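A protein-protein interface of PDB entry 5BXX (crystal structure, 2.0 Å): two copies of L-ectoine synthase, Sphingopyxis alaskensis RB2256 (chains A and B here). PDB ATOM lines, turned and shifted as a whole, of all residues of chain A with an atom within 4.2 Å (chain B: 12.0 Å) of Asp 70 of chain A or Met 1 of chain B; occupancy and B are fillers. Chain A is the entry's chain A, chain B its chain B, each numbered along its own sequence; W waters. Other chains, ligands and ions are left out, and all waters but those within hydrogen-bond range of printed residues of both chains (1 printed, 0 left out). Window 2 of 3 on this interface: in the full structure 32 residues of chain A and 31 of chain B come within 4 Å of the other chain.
Water W1 bridges OD2 of Asp 88 of chain A (2.6 Å) and O of Asp 31 of chain B (2.7 Å).
O of Ile 68 of chain A lies within hydrogen-bond range of N of His 77 of chain A (2.8 Å). The backbone NH (N) of Ala 72 of chain A sits at hydrogen-bond distance from the side-chain carboxylate (OD1) of Asp 70 of chain A (3.1 Å). The backbone NH (N) of Asp 70 of chain A sits at hydrogen-bond distance from the backbone carbonyl oxygen (O) of Glu 75 of chain A, at 3.0 Å. The backbone NH of Asp 88 of chain A lies within hydrogen-bond range of the side-chain carboxylate of Asp 91 of chain A (3.3 Å). The backbone NH (N) of Asp 89 of chain A is in hydrogen-bond range of the side-chain carboxylate (OD2) of Asp 91 of chain A (3.0 Å).
O of Ile 2 of chain B sits at hydrogen-bond distance from N of Ala 86 of chain A. The side-chain carboxylate (OD1) of Asp 88 of chain A lies within hydrogen-bond range of the backbone NH (N) of Met 1 of chain B, 2.8 Å away. The side-chain carboxylate of Asp 91 of chain A lies within hydrogen-bond range of the backbone NH of Met 1 of chain B (2.9 Å).
Among the printed residues, pairs that only touch across the chains: His 77 of chain A with Met 1 of chain B, Ala 86 of chain A with Met 1 of chain B, His 77 of chain A with Val 3 of chain B, Asp 89 of chain A with Met 1 of chain B, Asp 88 of chain A with Met 33 of chain B, Asp 88 of chain A with Ile 2 of chain B, Asp 70 of chain A with Met 1 of chain B and Ala 86 of chain A with Met 33 of chain B.
Of the 12 printed residues of chain B, 4 touch a printed residue of chain A. Printed residues of chain B that touch a printed residue of chain A: Met 1, Ile 2, Val 3 and Met 33. Hydrophobic or aromatic side chains of chain B that line the printed part of chain A: Met 1, Ile 2, Val 3 and Met 33. Among the printed residues, 11 pairs touch across the chains.
No position is printed for both chains. Of the 11 pairs that touch across the chains among the printed residues, none has its exchanged pair printed and touching as well.
No residue of chain B comes within 4 Å of Glu 69 of chain A. Asp 70 of chain A touches one residue of chain B. No residue of chain B comes within 4 Å of Ala 72 of chain A. No residue of chain B comes within 4 Å of Thr 73 of chain A. No residue of chain B comes within 4 Å of Gly 74 of chain A. No residue of chain B comes within 4 Å of Glu 75 of chain A. Of chain B, only Met 1 and Val 3 come within 4 Å of His 77 of chain A. Of chain B, only Met 1 (3.4 Å), Ile 2 (2.9 Å) and Met 33 (3.9 Å) come within 4 Å of Ala 86 of chain A. Of chain B, only Met 1 (3.6 Å) comes within 4 Å of Asp 89 of chain A. No residue of chain B comes within 4 Å of Arg 92 of chain A. Of the printed residues of chain A, Ile 2 of chain B touches Ala 86 and Asp 88. Of the printed residues of chain A, Val 3 of chain B touches His 77 (3.5 Å). Asp 30 of chain B touches none of the printed residues of chain A. Asp 31 of chain B touches none of the printed residues of chain A. Of the printed residues of chain A, Met 33 of chain B touches Ala 86 and Asp 88. The nearest residue of chain B that does not touch Asp 70 of chain A is Ile 2 of chain B (6.9 Å). The nearest printed residue of chain A that does not touch Ile 2 of chain B is Asp 91 of chain A (5.8 Å).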
ATOM      1  N   ILE A  68     -26.385  22.681  19.637  1.00  0.00           N
ATOM      2  CA  ILE A  68     -25.637  23.635  18.836  1.00  0.00           C
ATOM      3  C   ILE A  68     -24.981  22.905  17.627  1.00  0.00           C
ATOM      4  O   ILE A  68     -24.378  21.857  17.769  1.00  0.00           O
ATOM      5  CB  ILE A  68     -24.571  24.354  19.654  1.00  0.00           C
ATOM      6  CG1 ILE A  68     -23.855  25.430  18.805  1.00  0.00           C
ATOM      7  CG2 ILE A  68     -23.634  23.350  20.259  1.00  0.00           C
ATOM      8  CD1 ILE A  68     -22.979  26.340  19.572  1.00  0.00           C
ATOM      9  N   GLU A  69     -25.093  23.516  16.469  1.00  0.00           N
ATOM     10  CA  GLU A  69     -24.496  22.983  15.223  1.00  0.00           C
ATOM     11  C   GLU A  69     -23.337  23.843  14.783  1.00  0.00           C
ATOM     12  O   GLU A  69     -23.484  25.090  14.658  1.00  0.00           O
ATOM     13  CB  GLU A  69     -25.527  22.957  14.117  1.00  0.00           C
ATOM     14  CG  GLU A  69     -24.878  22.561  12.773  1.00  0.00           C
ATOM     15  CD  GLU A  69     -25.869  22.415  11.657  1.00  0.00           C
ATOM     16  OE1 GLU A  69     -27.060  22.772  11.852  1.00  0.00           O
ATOM     17  OE2 GLU A  69     -25.430  21.935  10.572  1.00  0.00           O
ATOM     18  N   ASP A  70     -22.176  23.216  14.593  1.00  0.00           N
ATOM     19  CA  ASP A  70     -21.029  23.862  13.957  1.00  0.00           C
ATOM     20  C   ASP A  70     -21.134  23.771  12.448  1.00  0.00           C
ATOM     21  O   ASP A  70     -21.075  22.667  11.892  1.00  0.00           O
ATOM     22  CB  ASP A  70     -19.743  23.246  14.470  1.00  0.00           C
ATOM     23  CG  ASP A  70     -18.485  23.877  13.874  1.00  0.00           C
ATOM     24  OD1 ASP A  70     -18.555  24.860  13.088  1.00  0.00           O
ATOM     25  OD2 ASP A  70     -17.396  23.426  14.287  1.00  0.00           O
ATOM     26  N   LEU A  71     -21.300  24.921  11.778  1.00  0.00           N
ATOM     27  CA  LEU A  71     -21.627  24.880  10.338  1.00  0.00           C
ATOM     28  C   LEU A  71     -20.395  24.637   9.477  1.00  0.00           C
ATOM     29  O   LEU A  71     -20.521  24.444   8.298  1.00  0.00           O
ATOM     30  CB  LEU A  71     -22.352  26.169   9.901  1.00  0.00           C
ATOM     31  CG  LEU A  71     -23.851  26.251  10.279  1.00  0.00           C
ATOM     32  CD1 LEU A  71     -24.525  27.490   9.752  1.00  0.00           C
ATOM     33  CD2 LEU A  71     -24.620  25.080   9.755  1.00  0.00           C
ATOM     34  N   ALA A  72     -19.215  24.593  10.072  1.00  0.00           N
ATOM     35  CA  ALA A  72     -18.012  24.225   9.334  1.00  0.00           C
ATOM     36  C   ALA A  72     -18.035  22.762   8.971  1.00  0.00           C
ATOM     37  O   ALA A  72     -17.408  22.354   8.006  1.00  0.00           O
ATOM     38  CB  ALA A  72     -16.778  24.521  10.149  1.00  0.00           C
ATOM     39  N   THR A  73     -18.743  21.973   9.769  1.00  0.00           N
ATOM     40  CA  THR A  73     -18.740  20.539   9.617  1.00  0.00           C
ATOM     41  C   THR A  73     -20.112  19.923   9.643  1.00  0.00           C
ATOM     42  O   THR A  73     -20.264  18.764   9.245  1.00  0.00           O
ATOM     43  CB  THR A  73     -17.899  19.856  10.722  1.00  0.00           C
ATOM     44  OG1 THR A  73     -18.541  19.993  11.985  1.00  0.00           O
ATOM     45  CG2 THR A  73     -16.505  20.442  10.800  1.00  0.00           C
ATOM     46  N   GLY A  74     -21.110  20.667  10.131  1.00  0.00           N
ATOM     47  CA  GLY A  74     -22.414  20.088  10.386  1.00  0.00           C
ATOM     48  C   GLY A  74     -22.522  19.293  11.675  1.00  0.00           C
ATOM     49  O   GLY A  74     -23.597  18.766  11.991  1.00  0.00           O
ATOM     50  N   GLU A  75     -21.437  19.170  12.431  1.00  0.00           N
ATOM     51  CA  GLU A  75     -21.534  18.433  13.692  1.00  0.00           C
ATOM     52  C   GLU A  75     -22.544  19.057  14.669  1.00  0.00           C
ATOM     53  O   GLU A  75     -22.590  20.270  14.831  1.00  0.00           O
ATOM     54  CB  GLU A  75     -20.188  18.327  14.407  1.00  0.00           C
ATOM     55  CG  GLU A  75     -20.335  17.512  15.700  1.00  0.00           C
ATOM     56  CD  GLU A  75     -19.020  17.143  16.380  1.00  0.00           C
ATOM     57  OE1 GLU A  75     -17.939  17.469  15.843  1.00  0.00           O
ATOM     58  OE2 GLU A  75     -19.087  16.495  17.444  1.00  0.00           O
ATOM     59  N   HIS A  77     -23.897  19.167  18.552  1.00  0.00           N
ATOM     60  CA  HIS A  77     -23.511  18.884  19.931  1.00  0.00           C
ATOM     61  C   HIS A  77     -24.702  19.063  20.886  1.00  0.00           C
ATOM     62  O   HIS A  77     -25.462  20.001  20.763  1.00  0.00           O
ATOM     63  CB  HIS A  77     -22.397  19.803  20.371  1.00  0.00           C
ATOM     64  CG  HIS A  77     -21.224  19.887  19.430  1.00  0.00           C
ATOM     65  ND1 HIS A  77     -20.010  19.314  19.722  1.00  0.00           N
ATOM     66  CD2 HIS A  77     -21.053  20.557  18.259  1.00  0.00           C
ATOM     67  CE1 HIS A  77     -19.149  19.591  18.755  1.00  0.00           C
ATOM     68  NE2 HIS A  77     -19.754  20.353  17.857  1.00  0.00           N
ATOM     69  N   ALA A  86     -17.326  27.315  23.369  1.00  0.00           N
ATOM     70  CA  ALA A  86     -16.567  28.512  23.032  1.00  0.00           C
ATOM     71  C   ALA A  86     -16.406  28.665  21.525  1.00  0.00           C
ATOM     72  O   ALA A  86     -15.984  27.737  20.867  1.00  0.00           O
ATOM     73  CB  ALA A  86     -15.209  28.450  23.674  1.00  0.00           C
ATOM     74  N   ASP A  88     -14.275  29.879  19.445  1.00  0.00           N
ATOM     75  CA  ASP A  88     -12.896  30.363  19.370  1.00  0.00           C
ATOM     76  C   ASP A  88     -12.418  30.663  17.933  1.00  0.00           C
ATOM     77  O   ASP A  88     -11.351  31.235  17.741  1.00  0.00           O
ATOM     78  CB  ASP A  88     -11.967  29.336  20.025  1.00  0.00           C
ATOM     79  CG  ASP A  88     -12.001  27.966  19.298  1.00  0.00           C
ATOM     80  OD1 ASP A  88     -13.079  27.597  18.770  1.00  0.00           O
ATOM     81  OD2 ASP A  88     -10.954  27.270  19.270  1.00  0.00           O
ATOM     82  N   ASP A  89     -13.192  30.244  16.923  1.00  0.00           N
ATOM     83  CA  ASP A  89     -12.808  30.426  15.512  1.00  0.00           C
ATOM     84  C   ASP A  89     -13.772  31.383  14.824  1.00  0.00           C
ATOM     85  O   ASP A  89     -13.989  31.312  13.624  1.00  0.00           O
ATOM     86  CB  ASP A  89     -12.783  29.066  14.758  1.00  0.00           C
ATOM     87  CG  ASP A  89     -11.661  28.137  15.240  1.00  0.00           C
ATOM     88  OD1 ASP A  89     -10.620  28.674  15.684  1.00  0.00           O
ATOM     89  OD2 ASP A  89     -11.816  26.883  15.195  1.00  0.00           O
ATOM     90  N   ASP A  91     -16.897  31.012  14.955  1.00  0.00           N
ATOM     91  CA  ASP A  91     -17.636  29.949  14.266  1.00  0.00           C
ATOM     92  C   ASP A  91     -19.021  30.387  13.874  1.00  0.00           C
ATOM     93  O   ASP A  91     -19.691  31.137  14.597  1.00  0.00           O
ATOM     94  CB  ASP A  91     -17.724  28.711  15.136  1.00  0.00           C
ATOM     95  CG  ASP A  91     -16.396  28.360  15.765  1.00  0.00           C
ATOM     96  OD1 ASP A  91     -15.839  27.326  15.400  1.00  0.00           O
ATOM     97  OD2 ASP A  91     -15.904  29.108  16.644  1.00  0.00           O
ATOM     98  N   ARG A  92     -19.442  29.919  12.697  1.00  0.00           N
ATOM     99  CA  ARG A  92     -20.796  30.123  12.256  1.00  0.00           C
ATOM    100  C   ARG A  92     -21.539  28.993  12.914  1.00  0.00           C
ATOM    101  O   ARG A  92     -21.143  27.832  12.735  1.00  0.00           O
ATOM    102  CB  ARG A  92     -20.905  30.054  10.720  1.00  0.00           C
ATOM    103  CG  ARG A  92     -20.224  31.197   9.953  1.00  0.00           C
ATOM    104  CD  ARG A  92     -20.382  31.002   8.443  1.00  0.00           C
ATOM    105  NE  ARG A  92     -19.898  29.668   8.067  1.00  0.00           N
ATOM    106  CZ  ARG A  92     -20.639  28.683   7.521  1.00  0.00           C
ATOM    107  NH1 ARG A  92     -21.926  28.840   7.225  1.00  0.00           N
ATOM    108  NH2 ARG A  92     -20.082  27.512   7.252  1.00  0.00           N
ATOM    109  N   MET B   1     -14.419  25.636  17.313  1.00  0.00           N
ATOM    110  CA  MET B   1     -15.476  25.510  18.341  1.00  0.00           C
ATOM    111  C   MET B   1     -14.970  24.556  19.392  1.00  0.00           C
ATOM    112  O   MET B   1     -14.469  23.483  19.071  1.00  0.00           O
ATOM    113  CB  MET B   1     -16.790  25.018  17.752  1.00  0.00           C
ATOM    114  CG  MET B   1     -17.950  25.168  18.691  1.00  0.00           C
ATOM    115  SD  MET B   1     -19.528  24.875  17.899  1.00  0.00           S
ATOM    116  CE  MET B   1     -19.852  23.498  18.864  1.00  0.00           C
ATOM    117  N   ILE B   2     -15.077  24.960  20.651  1.00  0.00           N
ATOM    118  CA  ILE B   2     -14.673  24.094  21.751  1.00  0.00           C
ATOM    119  C   ILE B   2     -15.957  23.718  22.448  1.00  0.00           C
ATOM    120  O   ILE B   2     -16.778  24.588  22.677  1.00  0.00           O
ATOM    121  CB  ILE B   2     -13.677  24.800  22.697  1.00  0.00           C
ATOM    122  CG1 ILE B   2     -12.379  25.063  21.946  1.00  0.00           C
ATOM    123  CG2 ILE B   2     -13.384  23.953  23.943  1.00  0.00           C
ATOM    124  CD1 ILE B   2     -11.425  26.069  22.696  1.00  0.00           C
ATOM    125  N   VAL B   3     -16.159  22.427  22.727  1.00  0.00           N
ATOM    126  CA  VAL B   3     -17.326  21.985  23.497  1.00  0.00           C
ATOM    127  C   VAL B   3     -16.827  21.061  24.591  1.00  0.00           C
ATOM    128  O   VAL B   3     -16.202  20.049  24.293  1.00  0.00           O
ATOM    129  CB  VAL B   3     -18.378  21.242  22.644  1.00  0.00           C
ATOM    130  CG1 VAL B   3     -19.576  20.804  23.514  1.00  0.00           C
ATOM    131  CG2 VAL B   3     -18.831  22.124  21.477  1.00  0.00           C
ATOM    132  N   ARG B   4     -17.063  21.440  25.852  1.00  0.00           N
ATOM    133  CA  ARG B   4     -16.689  20.591  26.966  1.00  0.00           C
ATOM    134  C   ARG B   4     -17.855  20.509  27.906  1.00  0.00           C
ATOM    135  O   ARG B   4     -18.899  21.075  27.643  1.00  0.00           O
ATOM    136  CB  ARG B   4     -15.440  21.111  27.645  1.00  0.00           C
ATOM    137  CG  ARG B   4     -14.379  21.472  26.622  1.00  0.00           C
ATOM    138  CD  ARG B   4     -12.952  21.419  27.127  1.00  0.00           C
ATOM    139  NE  ARG B   4     -12.387  22.721  27.278  1.00  0.00           N
ATOM    140  CZ  ARG B   4     -11.289  23.186  26.687  1.00  0.00           C
ATOM    141  NH1 ARG B   4     -10.559  22.496  25.837  1.00  0.00           N
ATOM    142  NH2 ARG B   4     -10.905  24.403  26.988  1.00  0.00           N
ATOM    143  N   ASN B   5     -17.708  19.735  28.968  1.00  0.00           N
ATOM    144  CA  ASN B   5     -18.756  19.644  29.949  1.00  0.00           C
ATOM    145  C   ASN B   5     -18.137  19.389  31.306  1.00  0.00           C
ATOM    146  O   ASN B   5     -17.108  18.717  31.429  1.00  0.00           O
ATOM    147  CB  ASN B   5     -19.754  18.562  29.609  1.00  0.00           C
ATOM    148  CG  ASN B   5     -19.147  17.197  29.696  1.00  0.00           C
ATOM    149  OD1 ASN B   5     -19.214  16.565  30.729  1.00  0.00           O
ATOM    150  ND2 ASN B   5     -18.500  16.751  28.617  1.00  0.00           N
ATOM    151  N   ARG B  14      -7.735  19.541  34.902  1.00  0.00           N
ATOM    152  CA  ARG B  14      -8.181  20.899  34.764  1.00  0.00           C
ATOM    153  C   ARG B  14      -9.184  21.173  35.867  1.00  0.00           C
ATOM    154  O   ARG B  14      -9.712  22.259  35.956  1.00  0.00           O
ATOM    155  CB  ARG B  14      -8.741  21.163  33.366  1.00  0.00           C
ATOM    156  CG  ARG B  14      -7.617  21.624  32.413  1.00  0.00           C
ATOM    157  CD  ARG B  14      -8.139  22.294  31.175  1.00  0.00           C
ATOM    158  NE  ARG B  14      -9.223  21.495  30.601  1.00  0.00           N
ATOM    159  CZ  ARG B  14      -9.170  20.799  29.458  1.00  0.00           C
ATOM    160  NH1 ARG B  14      -8.081  20.790  28.684  1.00  0.00           N
ATOM    161  NH2 ARG B  14     -10.237  20.108  29.075  1.00  0.00           N
ATOM    162  N   MET B  26     -13.004  25.373  32.665  1.00  0.00           N
ATOM    163  CA  MET B  26     -13.630  25.116  31.399  1.00  0.00           C
ATOM    164  C   MET B  26     -12.792  25.681  30.260  1.00  0.00           C
ATOM    165  O   MET B  26     -12.756  25.130  29.151  1.00  0.00           O
ATOM    166  CB  MET B  26     -15.050  25.727  31.369  1.00  0.00           C
ATOM    167  CG  MET B  26     -16.065  25.351  32.509  1.00  0.00           C
ATOM    168  SD  MET B  26     -16.096  23.609  32.847  1.00  0.00           S
ATOM    169  CE  MET B  26     -17.042  23.000  31.431  1.00  0.00           C
ATOM    170  N   LEU B  27     -12.128  26.797  30.524  1.00  0.00           N
ATOM    171  CA  LEU B  27     -11.214  27.431  29.575  1.00  0.00           C
ATOM    172  C   LEU B  27     -10.022  28.017  30.230  1.00  0.00           C
ATOM    173  O   LEU B  27     -10.180  28.702  31.231  1.00  0.00           O
ATOM    174  CB  LEU B  27     -11.841  28.588  28.857  1.00  0.00           C
ATOM    175  CG  LEU B  27     -12.966  28.441  27.915  1.00  0.00           C
ATOM    176  CD1 LEU B  27     -13.308  29.856  27.588  1.00  0.00           C
ATOM    177  CD2 LEU B  27     -12.504  27.583  26.640  1.00  0.00           C
ATOM    178  N   ASP B  30      -4.646  28.872  27.204  1.00  0.00           N
ATOM    179  CA  ASP B  30      -4.231  28.143  25.983  1.00  0.00           C
ATOM    180  C   ASP B  30      -5.334  28.066  24.948  1.00  0.00           C
ATOM    181  O   ASP B  30      -5.073  27.860  23.786  1.00  0.00           O
ATOM    182  CB  ASP B  30      -3.787  26.713  26.319  1.00  0.00           C
ATOM    183  CG  ASP B  30      -2.348  26.638  26.804  1.00  0.00           C
ATOM    184  OD1 ASP B  30      -1.799  27.695  27.226  1.00  0.00           O
ATOM    185  OD2 ASP B  30      -1.773  25.519  26.774  1.00  0.00           O
ATOM    186  N   ASP B  31      -6.573  28.200  25.404  1.00  0.00           N
ATOM    187  CA  ASP B  31      -7.739  28.082  24.574  1.00  0.00           C
ATOM    188  C   ASP B  31      -7.945  29.309  23.719  1.00  0.00           C
ATOM    189  O   ASP B  31      -8.796  29.312  22.792  1.00  0.00           O
ATOM    190  CB  ASP B  31      -8.948  27.804  25.464  1.00  0.00           C
ATOM    191  CG  ASP B  31      -8.919  26.398  26.016  1.00  0.00           C
ATOM    192  OD1 ASP B  31      -8.676  25.444  25.221  1.00  0.00           O
ATOM    193  OD2 ASP B  31      -9.099  26.221  27.237  1.00  0.00           O
ATOM    194  N   GLY B  32      -7.185  30.356  24.029  1.00  0.00           N
ATOM    195  CA  GLY B  32      -7.133  31.564  23.213  1.00  0.00           C
ATOM    196  C   GLY B  32      -8.321  32.522  23.197  1.00  0.00           C
ATOM    197  O   GLY B  32      -8.482  33.292  22.247  1.00  0.00           O
ATOM    198  N   MET B  33      -9.172  32.477  24.214  1.00  0.00           N
ATOM    199  CA  MET B  33     -10.354  33.352  24.241  1.00  0.00           C
ATOM    200  C   MET B  33     -10.023  34.710  24.857  1.00  0.00           C
ATOM    201  O   MET B  33     -10.776  35.665  24.710  1.00  0.00           O
ATOM    202  CB  MET B  33     -11.469  32.687  25.039  1.00  0.00           C
ATOM    203  CG  MET B  33     -11.877  31.324  24.548  1.00  0.00           C
ATOM    204  SD  MET B  33     -12.546  31.464  22.893  1.00  0.00           S
ATOM    205  CE  MET B  33     -14.166  32.118  23.105  1.00  0.00           C
HETATM  206  O   HOH W   1      -8.780  27.712  20.659  1.00  0.00           O
